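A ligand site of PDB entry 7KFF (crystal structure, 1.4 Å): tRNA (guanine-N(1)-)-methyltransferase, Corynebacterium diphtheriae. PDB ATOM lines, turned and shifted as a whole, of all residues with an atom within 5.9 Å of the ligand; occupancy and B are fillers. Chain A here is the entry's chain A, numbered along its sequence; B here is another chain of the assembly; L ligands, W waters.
N4 of the ligand sits at hydrogen-bond distance from O of Tyr 194.
An oxygen (O5) of the ligand is in hydrogen-bond range of the backbone carbonyl oxygen (O) of Pro 141.
N of Gly 199 sits at hydrogen-bond distance from O5 of the ligand, at 3.4 Å.
The side-chain carboxylate (OE2) of Glu 170 lies within salt-bridge range of a nitrogen (N1) of the ligand (3.4 Å).
N6 of the ligand is in hydrogen-bond range of N of Thr 142 (3.4 Å).
N of Ser 228 of chain B sits at hydrogen-bond distance from O1 of the ligand, 2.7 Å away.
N of Gly 198 sits close to O3 of the ligand (3.4 Å).
The side-chain carboxylate of Asp 227 of chain B lies within salt-bridge range of a nitrogen (N1) of the ligand (3.0 Å).
A nitrogen (N4) of the ligand is in hydrogen-bond range of the backbone carbonyl oxygen (O) of Gly 192, at 3.0 Å.
OG of Ser 228 of chain B sits at hydrogen-bond distance from O2 of the ligand, 2.7 Å away.
A nitrogen (N4) of the ligand sits at hydrogen-bond distance from the side-chain hydroxyl of Ser 190, at 3.4 Å.
An oxygen (O5) of the ligand lies within hydrogen-bond range of the backbone NH (N) of Gly 167.
N of Leu 196 lies within hydrogen-bond range of N3 of the ligand (3.0 Å).
N of Ile 191 sits at hydrogen-bond distance from N5 of the ligand, 3.1 Å away.
OD1 of Asp 227 of chain B is in salt-bridge range of NH2 of Arg 212 of chain B (2.9 Å).
The side-chain carboxylate (OE1) of Glu 170 is in hydrogen-bond range of a ring nitrogen (NE2) of His 224 of chain B.
N of Thr 142 is in hydrogen-bond range of O of Val 189 (2.9 Å).
N of Ser 190 lies close to O of Thr 142 (3.3 Å).
The side-chain hydroxyl (OG) of Ser 228 of chain B is in hydrogen-bond range of the backbone NH (N) of Glu 235 of chain B (3.0 Å).
The side-chain hydroxyl of Thr 142 lies within hydrogen-bond range of the backbone NH of Ala 144 (3.0 Å).
O of Gly 192 sits at hydrogen-bond distance from OG of Ser 190 (2.9 Å).
The side-chain hydroxyl of Tyr 194 lies within hydrogen-bond range of the backbone carbonyl oxygen of Ile 191, 3.1 Å away.
A sulfur (S1) of the ligand sits close to the backbone carbonyl oxygen (O) of Tyr 169, at 3.8 Å.
Residues that only touch the ligand: Pro 143, Glu 235 of chain B, Ile 197, Gly 171, Val 189, Val 195 and Ala 202.
Hydrophobic or aromatic side chains that line the ligand: Pro 141, Pro 143, Ile 191, Leu 196 and Ala 202.
Within 4 Å of the ligand: Pro 141, Thr 142, Pro 143, Gly 167, Tyr 169, Glu 170, Gly 171, Val 189, Ser 190, Ile 191, Gly 192, Tyr 194, Val 195, Leu 196, Ile 197, Gly 198, Gly 199, Ala 202, Asp 227 of chain B, Ser 228 of chain B and Glu 235 of chain B.
Water W3 lies within hydrogen-bond range of the backbone carbonyl oxygen (O) of Pro 141 (2.7 Å), the backbone carbonyl oxygen (O) of Ala 165 (2.8 Å), the backbone NH (N) of Gly 167 (2.8 Å) and an oxygen (O5) of the ligand (3.1 Å).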
ATOM      1  N   PRO A 141     -14.784   8.138   3.998  1.00  0.00           N
ATOM      2  CA  PRO A 141     -13.395   8.133   3.506  1.00  0.00           C
ATOM      3  C   PRO A 141     -12.531   7.232   4.373  1.00  0.00           C
ATOM      4  O   PRO A 141     -12.579   7.271   5.611  1.00  0.00           O
ATOM      5  CB  PRO A 141     -12.994   9.602   3.614  1.00  0.00           C
ATOM      6  CG  PRO A 141     -14.269  10.362   3.528  1.00  0.00           C
ATOM      7  CD  PRO A 141     -15.283   9.514   4.237  1.00  0.00           C
ATOM      8  N   THR A 142     -11.730   6.394   3.704  1.00  0.00           N
ATOM      9  CA  THR A 142     -10.776   5.559   4.400  1.00  0.00           C
ATOM     10  C   THR A 142      -9.764   5.076   3.383  1.00  0.00           C
ATOM     11  O   THR A 142     -10.143   4.763   2.242  1.00  0.00           O
ATOM     12  CB  THR A 142     -11.417   4.351   5.078  1.00  0.00           C
ATOM     13  OG1 THR A 142     -10.392   3.395   5.304  1.00  0.00           O
ATOM     14  CG2 THR A 142     -12.513   3.726   4.276  1.00  0.00           C
ATOM     15  N   PRO A 143      -8.480   5.009   3.736  1.00  0.00           N
ATOM     16  CA  PRO A 143      -7.489   4.516   2.765  1.00  0.00           C
ATOM     17  C   PRO A 143      -7.670   3.041   2.462  1.00  0.00           C
ATOM     18  O   PRO A 143      -7.042   2.528   1.531  1.00  0.00           O
ATOM     19  CB  PRO A 143      -6.146   4.773   3.461  1.00  0.00           C
ATOM     20  CG  PRO A 143      -6.497   4.737   4.933  1.00  0.00           C
ATOM     21  CD  PRO A 143      -7.874   5.319   5.041  1.00  0.00           C
ATOM     22  N   ALA A 144      -8.496   2.339   3.252  1.00  0.00           N
ATOM     23  CA  ALA A 144      -8.823   0.941   3.023  1.00  0.00           C
ATOM     24  C   ALA A 144     -10.144   0.752   2.285  1.00  0.00           C
ATOM     25  O   ALA A 144     -10.643  -0.372   2.204  1.00  0.00           O
ATOM     26  CB  ALA A 144      -8.817   0.197   4.352  1.00  0.00           C
ATOM     27  N   ALA A 165     -19.073  10.826   6.587  1.00  0.00           N
ATOM     28  CA  ALA A 165     -18.612  10.575   7.947  1.00  0.00           C
ATOM     29  C   ALA A 165     -17.094  10.703   7.952  1.00  0.00           C
ATOM     30  O   ALA A 165     -16.405   9.839   7.402  1.00  0.00           O
ATOM     31  CB  ALA A 165     -19.048   9.196   8.421  1.00  0.00           C
ATOM     32  N   CYS A 166     -16.570  11.768   8.551  1.00  0.00           N
ATOM     33  CA  CYS A 166     -15.136  12.055   8.512  1.00  0.00           C
ATOM     34  C   CYS A 166     -14.381  11.441   9.672  1.00  0.00           C
ATOM     35  O   CYS A 166     -14.579  11.822  10.825  1.00  0.00           O
ATOM     36  CB  CYS A 166     -14.868  13.560   8.518  1.00  0.00           C
ATOM     37  SG  CYS A 166     -15.616  14.439   7.154  1.00  0.00           S
ATOM     38  N   GLY A 167     -13.457  10.525   9.363  1.00  0.00           N
ATOM     39  CA  GLY A 167     -12.638   9.930  10.392  1.00  0.00           C
ATOM     40  C   GLY A 167     -11.399  10.750  10.720  1.00  0.00           C
ATOM     41  O   GLY A 167     -10.929  11.551   9.919  1.00  0.00           O
ATOM     42  N   ARG A 168     -10.896  10.513  11.919  1.00  0.00           N
ATOM     43  CA  ARG A 168      -9.625  11.002  12.415  1.00  0.00           C
ATOM     44  C   ARG A 168      -9.023   9.845  13.224  1.00  0.00           C
ATOM     45  O   ARG A 168      -9.706   8.859  13.517  1.00  0.00           O
ATOM     46  CB  ARG A 168      -9.842  12.225  13.314  1.00  0.00           C
ATOM     47  CG  ARG A 168     -10.270  13.490  12.578  1.00  0.00           C
ATOM     48  CD  ARG A 168      -9.088  14.297  12.153  1.00  0.00           C
ATOM     49  NE  ARG A 168      -9.364  15.232  11.066  1.00  0.00           N
ATOM     50  CZ  ARG A 168      -8.478  16.094  10.591  1.00  0.00           C
ATOM     51  NH1 ARG A 168      -7.300  16.256  11.175  1.00  0.00           N
ATOM     52  NH2 ARG A 168      -8.764  16.826   9.529  1.00  0.00           N
ATOM     53  N   TYR A 169      -7.739   9.986  13.582  1.00  0.00           N
ATOM     54  CA  TYR A 169      -7.068   9.034  14.457  1.00  0.00           C
ATOM     55  C   TYR A 169      -6.973   7.697  13.722  1.00  0.00           C
ATOM     56  O   TYR A 169      -6.512   7.661  12.578  1.00  0.00           O
ATOM     57  CB  TYR A 169      -7.764   8.985  15.817  1.00  0.00           C
ATOM     58  CG  TYR A 169      -8.090  10.376  16.335  1.00  0.00           C
ATOM     59  CD1 TYR A 169      -7.155  11.420  16.278  1.00  0.00           C
ATOM     60  CD2 TYR A 169      -9.359  10.662  16.821  1.00  0.00           C
ATOM     61  CE1 TYR A 169      -7.477  12.695  16.730  1.00  0.00           C
ATOM     62  CE2 TYR A 169      -9.685  11.915  17.296  1.00  0.00           C
ATOM     63  CZ  TYR A 169      -8.745  12.933  17.232  1.00  0.00           C
ATOM     64  OH  TYR A 169      -9.065  14.186  17.685  1.00  0.00           O
ATOM     65  N   GLU A 170      -7.364   6.585  14.351  1.00  0.00           N
ATOM     66  CA  GLU A 170      -7.321   5.298  13.665  1.00  0.00           C
ATOM     67  C   GLU A 170      -8.522   5.080  12.771  1.00  0.00           C
ATOM     68  O   GLU A 170      -8.564   4.103  12.004  1.00  0.00           O
ATOM     69  CB  GLU A 170      -7.239   4.168  14.684  1.00  0.00           C
ATOM     70  CG  GLU A 170      -5.979   4.202  15.534  1.00  0.00           C
ATOM     71  CD  GLU A 170      -4.717   4.211  14.692  1.00  0.00           C
ATOM     72  OE1 GLU A 170      -3.951   5.193  14.789  1.00  0.00           O
ATOM     73  OE2 GLU A 170      -4.493   3.224  13.952  1.00  0.00           O
ATOM     74  N   GLY A 171      -9.517   5.966  12.856  1.00  0.00           N
ATOM     75  CA  GLY A 171     -10.733   5.830  12.090  1.00  0.00           C
ATOM     76  C   GLY A 171     -11.935   5.623  12.967  1.00  0.00           C
ATOM     77  O   GLY A 171     -11.900   5.873  14.177  1.00  0.00           O
ATOM     78  N   ILE A 172     -12.999   5.131  12.365  1.00  0.00           N
ATOM     79  CA  ILE A 172     -14.293   4.972  13.016  1.00  0.00           C
ATOM     80  C   ILE A 172     -14.509   3.493  13.311  1.00  0.00           C
ATOM     81  O   ILE A 172     -14.234   2.625  12.476  1.00  0.00           O
ATOM     82  CB  ILE A 172     -15.405   5.512  12.093  1.00  0.00           C
ATOM     83  CG1 ILE A 172     -15.175   7.005  11.783  1.00  0.00           C
ATOM     84  CG2 ILE A 172     -16.770   5.266  12.708  1.00  0.00           C
ATOM     85  CD1 ILE A 172     -16.119   7.547  10.740  1.00  0.00           C
ATOM     86  N   VAL A 189     -14.517   4.674   0.875  1.00  0.00           N
ATOM     87  CA  VAL A 189     -13.876   5.195  -0.332  1.00  0.00           C
ATOM     88  C   VAL A 189     -12.512   5.787  -0.003  1.00  0.00           C
ATOM     89  O   VAL A 189     -12.381   6.637   0.887  1.00  0.00           O
ATOM     90  CB  VAL A 189     -14.780   6.225  -1.045  1.00  0.00           C
ATOM     91  CG1 VAL A 189     -15.293   7.304  -0.099  1.00  0.00           C
ATOM     92  CG2 VAL A 189     -14.074   6.854  -2.242  1.00  0.00           C
ATOM     93  N   SER A 190     -11.497   5.342  -0.741  1.00  0.00           N
ATOM     94  CA  SER A 190     -10.169   5.915  -0.654  1.00  0.00           C
ATOM     95  C   SER A 190      -9.943   6.868  -1.826  1.00  0.00           C
ATOM     96  O   SER A 190     -10.269   6.544  -2.966  1.00  0.00           O
ATOM     97  CB  SER A 190      -9.105   4.826  -0.735  1.00  0.00           C
ATOM     98  OG  SER A 190      -7.841   5.467  -0.754  1.00  0.00           O
ATOM     99  N   ILE A 191      -9.335   8.030  -1.549  1.00  0.00           N
ATOM    100  CA  ILE A 191      -8.993   8.924  -2.660  1.00  0.00           C
ATOM    101  C   ILE A 191      -7.644   8.608  -3.305  1.00  0.00           C
ATOM    102  O   ILE A 191      -7.309   9.198  -4.347  1.00  0.00           O
ATOM    103  CB  ILE A 191      -9.143  10.428  -2.309  1.00  0.00           C
ATOM    104  CG1 ILE A 191      -8.149  10.847  -1.215  1.00  0.00           C
ATOM    105  CG2 ILE A 191     -10.589  10.726  -1.950  1.00  0.00           C
ATOM    106  CD1 ILE A 191      -7.938  12.349  -1.155  1.00  0.00           C
ATOM    107  N   GLY A 192      -6.881   7.678  -2.743  1.00  0.00           N
ATOM    108  CA  GLY A 192      -5.609   7.287  -3.338  1.00  0.00           C
ATOM    109  C   GLY A 192      -4.772   6.507  -2.356  1.00  0.00           C
ATOM    110  O   GLY A 192      -5.092   6.410  -1.162  1.00  0.00           O
ATOM    111  N   ASP A 193      -3.659   5.978  -2.871  1.00  0.00           N
ATOM    112  CA  ASP A 193      -2.810   5.062  -2.096  1.00  0.00           C
ATOM    113  C   ASP A 193      -1.765   5.868  -1.316  1.00  0.00           C
ATOM    114  O   ASP A 193      -0.555   5.796  -1.536  1.00  0.00           O
ATOM    115  CB  ASP A 193      -2.169   4.011  -2.990  1.00  0.00           C
ATOM    116  CG  ASP A 193      -3.162   2.971  -3.528  1.00  0.00           C
ATOM    117  OD1 ASP A 193      -4.367   2.996  -3.186  1.00  0.00           O
ATOM    118  OD2 ASP A 193      -2.706   2.093  -4.295  1.00  0.00           O
ATOM    119  N   TYR A 194      -2.267   6.642  -0.365  1.00  0.00           N
ATOM    120  CA  TYR A 194      -1.445   7.478   0.487  1.00  0.00           C
ATOM    121  C   TYR A 194      -2.279   7.744   1.733  1.00  0.00           C
ATOM    122  O   TYR A 194      -3.492   7.514   1.735  1.00  0.00           O
ATOM    123  CB  TYR A 194      -1.020   8.780  -0.211  1.00  0.00           C
ATOM    124  CG  TYR A 194      -2.119   9.425  -1.007  1.00  0.00           C
ATOM    125  CD1 TYR A 194      -3.093  10.180  -0.389  1.00  0.00           C
ATOM    126  CD2 TYR A 194      -2.183   9.265  -2.385  1.00  0.00           C
ATOM    127  CE1 TYR A 194      -4.125  10.763  -1.128  1.00  0.00           C
ATOM    128  CE2 TYR A 194      -3.174   9.858  -3.127  1.00  0.00           C
ATOM    129  CZ  TYR A 194      -4.154  10.613  -2.487  1.00  0.00           C
ATOM    130  OH  TYR A 194      -5.166  11.188  -3.179  1.00  0.00           O
ATOM    131  N   VAL A 195      -1.615   8.174   2.801  1.00  0.00           N
ATOM    132  CA  VAL A 195      -2.253   8.264   4.104  1.00  0.00           C
ATOM    133  C   VAL A 195      -2.421   9.728   4.507  1.00  0.00           C
ATOM    134  O   VAL A 195      -1.438  10.467   4.622  1.00  0.00           O
ATOM    135  CB  VAL A 195      -1.490   7.475   5.173  1.00  0.00           C
ATOM    136  CG1 VAL A 195      -2.219   7.569   6.502  1.00  0.00           C
ATOM    137  CG2 VAL A 195      -1.249   6.015   4.735  1.00  0.00           C
ATOM    138  N   LEU A 196      -3.672  10.132   4.708  1.00  0.00           N
ATOM    139  CA  LEU A 196      -4.039  11.463   5.138  1.00  0.00           C
ATOM    140  C   LEU A 196      -4.205  11.507   6.654  1.00  0.00           C
ATOM    141  O   LEU A 196      -4.153  10.490   7.338  1.00  0.00           O
ATOM    142  CB  LEU A 196      -5.354  11.872   4.491  1.00  0.00           C
ATOM    143  CG  LEU A 196      -5.341  11.736   2.972  1.00  0.00           C
ATOM    144  CD1 LEU A 196      -6.730  11.960   2.425  1.00  0.00           C
ATOM    145  CD2 LEU A 196      -4.318  12.661   2.343  1.00  0.00           C
ATOM    146  N   ILE A 197      -4.471  12.711   7.165  1.00  0.00           N
ATOM    147  CA  ILE A 197      -4.699  12.905   8.601  1.00  0.00           C
ATOM    148  C   ILE A 197      -6.167  12.690   8.959  1.00  0.00           C
ATOM    149  O   ILE A 197      -6.506  12.159  10.027  1.00  0.00           O
ATOM    150  CB  ILE A 197      -4.210  14.304   9.041  1.00  0.00           C
ATOM    151  CG1 ILE A 197      -2.738  14.530   8.701  1.00  0.00           C
ATOM    152  CG2 ILE A 197      -4.477  14.519  10.535  1.00  0.00           C
ATOM    153  CD1 ILE A 197      -2.291  15.969   8.735  1.00  0.00           C
ATOM    154  N   GLY A 198      -7.071  13.133   8.091  1.00  0.00           N
ATOM    155  CA  GLY A 198      -8.481  13.034   8.370  1.00  0.00           C
ATOM    156  C   GLY A 198      -9.280  12.923   7.092  1.00  0.00           C
ATOM    157  O   GLY A 198      -8.775  13.170   5.987  1.00  0.00           O
ATOM    158  N   GLY A 199     -10.536  12.552   7.252  1.00  0.00           N
ATOM    159  CA  GLY A 199     -11.433  12.435   6.109  1.00  0.00           C
ATOM    160  C   GLY A 199     -11.950  13.729   5.529  1.00  0.00           C
ATOM    161  O   GLY A 199     -12.459  13.721   4.402  1.00  0.00           O
ATOM    162  N   GLU A 200     -11.808  14.846   6.241  1.00  0.00           N
ATOM    163  CA  GLU A 200     -12.361  16.119   5.767  1.00  0.00           C
ATOM    164  C   GLU A 200     -11.821  16.508   4.381  1.00  0.00           C
ATOM    165  O   GLU A 200     -12.596  16.928   3.512  1.00  0.00           O
ATOM    166  CB  GLU A 200     -12.056  17.223   6.770  1.00  0.00           C
ATOM    167  CG  GLU A 200     -12.808  17.075   8.116  1.00  0.00           C
ATOM    168  CD  GLU A 200     -12.227  16.079   9.116  1.00  0.00           C
ATOM    169  OE1 GLU A 200     -11.181  15.434   8.868  1.00  0.00           O
ATOM    170  OE2 GLU A 200     -12.864  15.948  10.182  1.00  0.00           O
ATOM    171  N   ALA A 202     -10.716  14.605   2.102  1.00  0.00           N
ATOM    172  CA  ALA A 202     -11.280  13.699   1.103  1.00  0.00           C
ATOM    173  C   ALA A 202     -12.700  14.091   0.739  1.00  0.00           C
ATOM    174  O   ALA A 202     -13.093  13.915  -0.422  1.00  0.00           O
ATOM    175  CB  ALA A 202     -11.235  12.271   1.640  1.00  0.00           C
ATOM    176  N   ARG B 212       2.274  15.208   7.987  1.00  0.00           N
ATOM    177  CA  ARG B 212       2.097  14.238   9.066  1.00  0.00           C
ATOM    178  C   ARG B 212       3.322  13.342   9.257  1.00  0.00           C
ATOM    179  O   ARG B 212       3.402  12.658  10.280  1.00  0.00           O
ATOM    180  CB  ARG B 212       0.857  13.390   8.874  1.00  0.00           C
ATOM    181  CG  ARG B 212       0.935  12.408   7.746  1.00  0.00           C
ATOM    182  CD  ARG B 212      -0.348  11.596   7.578  1.00  0.00           C
ATOM    183  NE  ARG B 212      -0.593  10.569   8.593  1.00  0.00           N
ATOM    184  CZ  ARG B 212      -0.058   9.359   8.597  1.00  0.00           C
ATOM    185  NH1 ARG B 212       0.816   8.990   7.684  1.00  0.00           N
ATOM    186  NH2 ARG B 212      -0.391   8.497   9.539  1.00  0.00           N
ATOM    187  N   HIS B 224       2.896   6.390  15.716  1.00  0.00           N
ATOM    188  CA  HIS B 224       3.334   5.030  15.423  1.00  0.00           C
ATOM    189  C   HIS B 224       3.385   4.716  13.931  1.00  0.00           C
ATOM    190  O   HIS B 224       2.376   4.781  13.222  1.00  0.00           O
ATOM    191  CB  HIS B 224       2.413   4.028  16.141  1.00  0.00           C
ATOM    192  CG  HIS B 224       0.949   4.303  15.958  1.00  0.00           C
ATOM    193  ND1 HIS B 224       0.272   5.255  16.690  1.00  0.00           N
ATOM    194  CD2 HIS B 224       0.041   3.750  15.122  1.00  0.00           C
ATOM    195  CE1 HIS B 224      -0.997   5.273  16.310  1.00  0.00           C
ATOM    196  NE2 HIS B 224      -1.158   4.371  15.366  1.00  0.00           N
ATOM    197  N   ASP B 227       0.427   1.479   9.240  1.00  0.00           N
ATOM    198  CA  ASP B 227      -0.640   2.181   8.530  1.00  0.00           C
ATOM    199  C   ASP B 227      -0.982   1.428   7.251  1.00  0.00           C
ATOM    200  O   ASP B 227      -0.291   0.484   6.888  1.00  0.00           O
ATOM    201  CB  ASP B 227      -0.223   3.614   8.175  1.00  0.00           C
ATOM    202  CG  ASP B 227      -0.471   4.593   9.317  1.00  0.00           C
ATOM    203  OD1 ASP B 227       0.204   5.660   9.359  1.00  0.00           O
ATOM    204  OD2 ASP B 227      -1.345   4.317  10.177  1.00  0.00           O
ATOM    205  N   SER B 228      -2.029   1.844   6.539  1.00  0.00           N
ATOM    206  CA  SER B 228      -2.347   1.180   5.278  1.00  0.00           C
ATOM    207  C   SER B 228      -1.199   1.357   4.304  1.00  0.00           C
ATOM    208  O   SER B 228      -0.551   2.411   4.261  1.00  0.00           O
ATOM    209  CB  SER B 228      -3.622   1.799   4.684  1.00  0.00           C
ATOM    210  OG  SER B 228      -4.787   1.285   5.313  1.00  0.00           O
ATOM    211  N   PHE B 229      -0.961   0.332   3.494  1.00  0.00           N
ATOM    212  CA  PHE B 229       0.055   0.245   2.453  1.00  0.00           C
ATOM    213  C   PHE B 229       1.437  -0.029   3.012  1.00  0.00           C
ATOM    214  O   PHE B 229       2.347  -0.313   2.233  1.00  0.00           O
ATOM    215  CB  PHE B 229       0.110   1.484   1.529  1.00  0.00           C
ATOM    216  CG  PHE B 229      -1.234   1.959   1.110  1.00  0.00           C
ATOM    217  CD1 PHE B 229      -2.020   1.175   0.289  1.00  0.00           C
ATOM    218  CD2 PHE B 229      -1.747   3.170   1.567  1.00  0.00           C
ATOM    219  CE1 PHE B 229      -3.285   1.587  -0.079  1.00  0.00           C
ATOM    220  CE2 PHE B 229      -3.006   3.570   1.219  1.00  0.00           C
ATOM    221  CZ  PHE B 229      -3.780   2.774   0.397  1.00  0.00           C
ATOM    222  N   GLU B 235      -5.238  -1.657   5.805  1.00  0.00           N
ATOM    223  CA  GLU B 235      -5.519  -1.922   7.212  1.00  0.00           C
ATOM    224  C   GLU B 235      -6.924  -2.497   7.373  1.00  0.00           C
ATOM    225  O   GLU B 235      -7.856  -2.143   6.652  1.00  0.00           O
ATOM    226  CB  GLU B 235      -5.410  -0.649   8.042  1.00  0.00           C
ATOM    227  CG  GLU B 235      -3.976  -0.246   8.403  1.00  0.00           C
ATOM    228  CD  GLU B 235      -3.341  -1.118   9.485  1.00  0.00           C
ATOM    229  OE1 GLU B 235      -2.109  -1.345   9.419  1.00  0.00           O
ATOM    230  OE2 GLU B 235      -4.062  -1.573  10.414  1.00  0.00           O
HETATM  231  N1  LIG L   1      -4.293   3.690  10.617  1.00  0.00           N
HETATM  232  C1  LIG L   1      -5.096   4.087   9.476  1.00  0.00           C
HETATM  233  C2  LIG L   1      -4.995   5.587   9.367  1.00  0.00           C
HETATM  234  C3  LIG L   1      -6.308   6.341   9.498  1.00  0.00           C
HETATM  235  S1  LIG L   1      -5.937   7.950   8.839  1.00  0.00           S
HETATM  236  C4  LIG L   1      -4.632   3.477   8.159  1.00  0.00           C
HETATM  237  O1  LIG L   1      -3.510   3.725   7.709  1.00  0.00           O
HETATM  238  O2  LIG L   1      -5.388   2.759   7.502  1.00  0.00           O
HETATM  239  C5  LIG L   1      -7.289   8.836   9.587  1.00  0.00           C
HETATM  240  C6  LIG L   1      -8.464   9.089   8.658  1.00  0.00           C
HETATM  241  O3  LIG L   1      -8.066   9.891   7.545  1.00  0.00           O
HETATM  242  C7  LIG L   1      -9.149   7.867   8.040  1.00  0.00           C
HETATM  243  O4  LIG L   1      -9.963   7.218   8.948  1.00  0.00           O
HETATM  244  C8  LIG L   1      -9.885   8.519   6.866  1.00  0.00           C
HETATM  245  O5  LIG L   1     -11.048   9.186   7.300  1.00  0.00           O
HETATM  246  C9  LIG L   1      -8.866   9.557   6.424  1.00  0.00           C
HETATM  247  N2  LIG L   1      -7.975   9.052   5.365  1.00  0.00           N
HETATM  248  C10 LIG L   1      -6.627   8.790   5.466  1.00  0.00           C
HETATM  249  N3  LIG L   1      -6.156   8.436   4.261  1.00  0.00           N
HETATM  250  C11 LIG L   1      -7.198   8.447   3.392  1.00  0.00           C
HETATM  251  C12 LIG L   1      -7.302   8.161   2.033  1.00  0.00           C
HETATM  252  N4  LIG L   1      -6.274   7.756   1.266  1.00  0.00           N
HETATM  253  N5  LIG L   1      -8.539   8.289   1.437  1.00  0.00           N
HETATM  254  C13 LIG L   1      -9.631   8.696   2.169  1.00  0.00           C
HETATM  255  N6  LIG L   1      -9.530   8.998   3.494  1.00  0.00           N
HETATM  256  C14 LIG L   1      -8.332   8.865   4.080  1.00  0.00           C
HETATM  257  O   HOH W   1      -9.646   4.537   8.634  1.00  0.00           O
HETATM  258  O   HOH W   2     -12.729   6.556   9.160  1.00  0.00           O
HETATM  259  O   HOH W   3     -14.033   8.374   7.589  1.00  0.00           O
HETATM  260  O   HOH W   4      -7.885   2.553   7.987  1.00  0.00           O
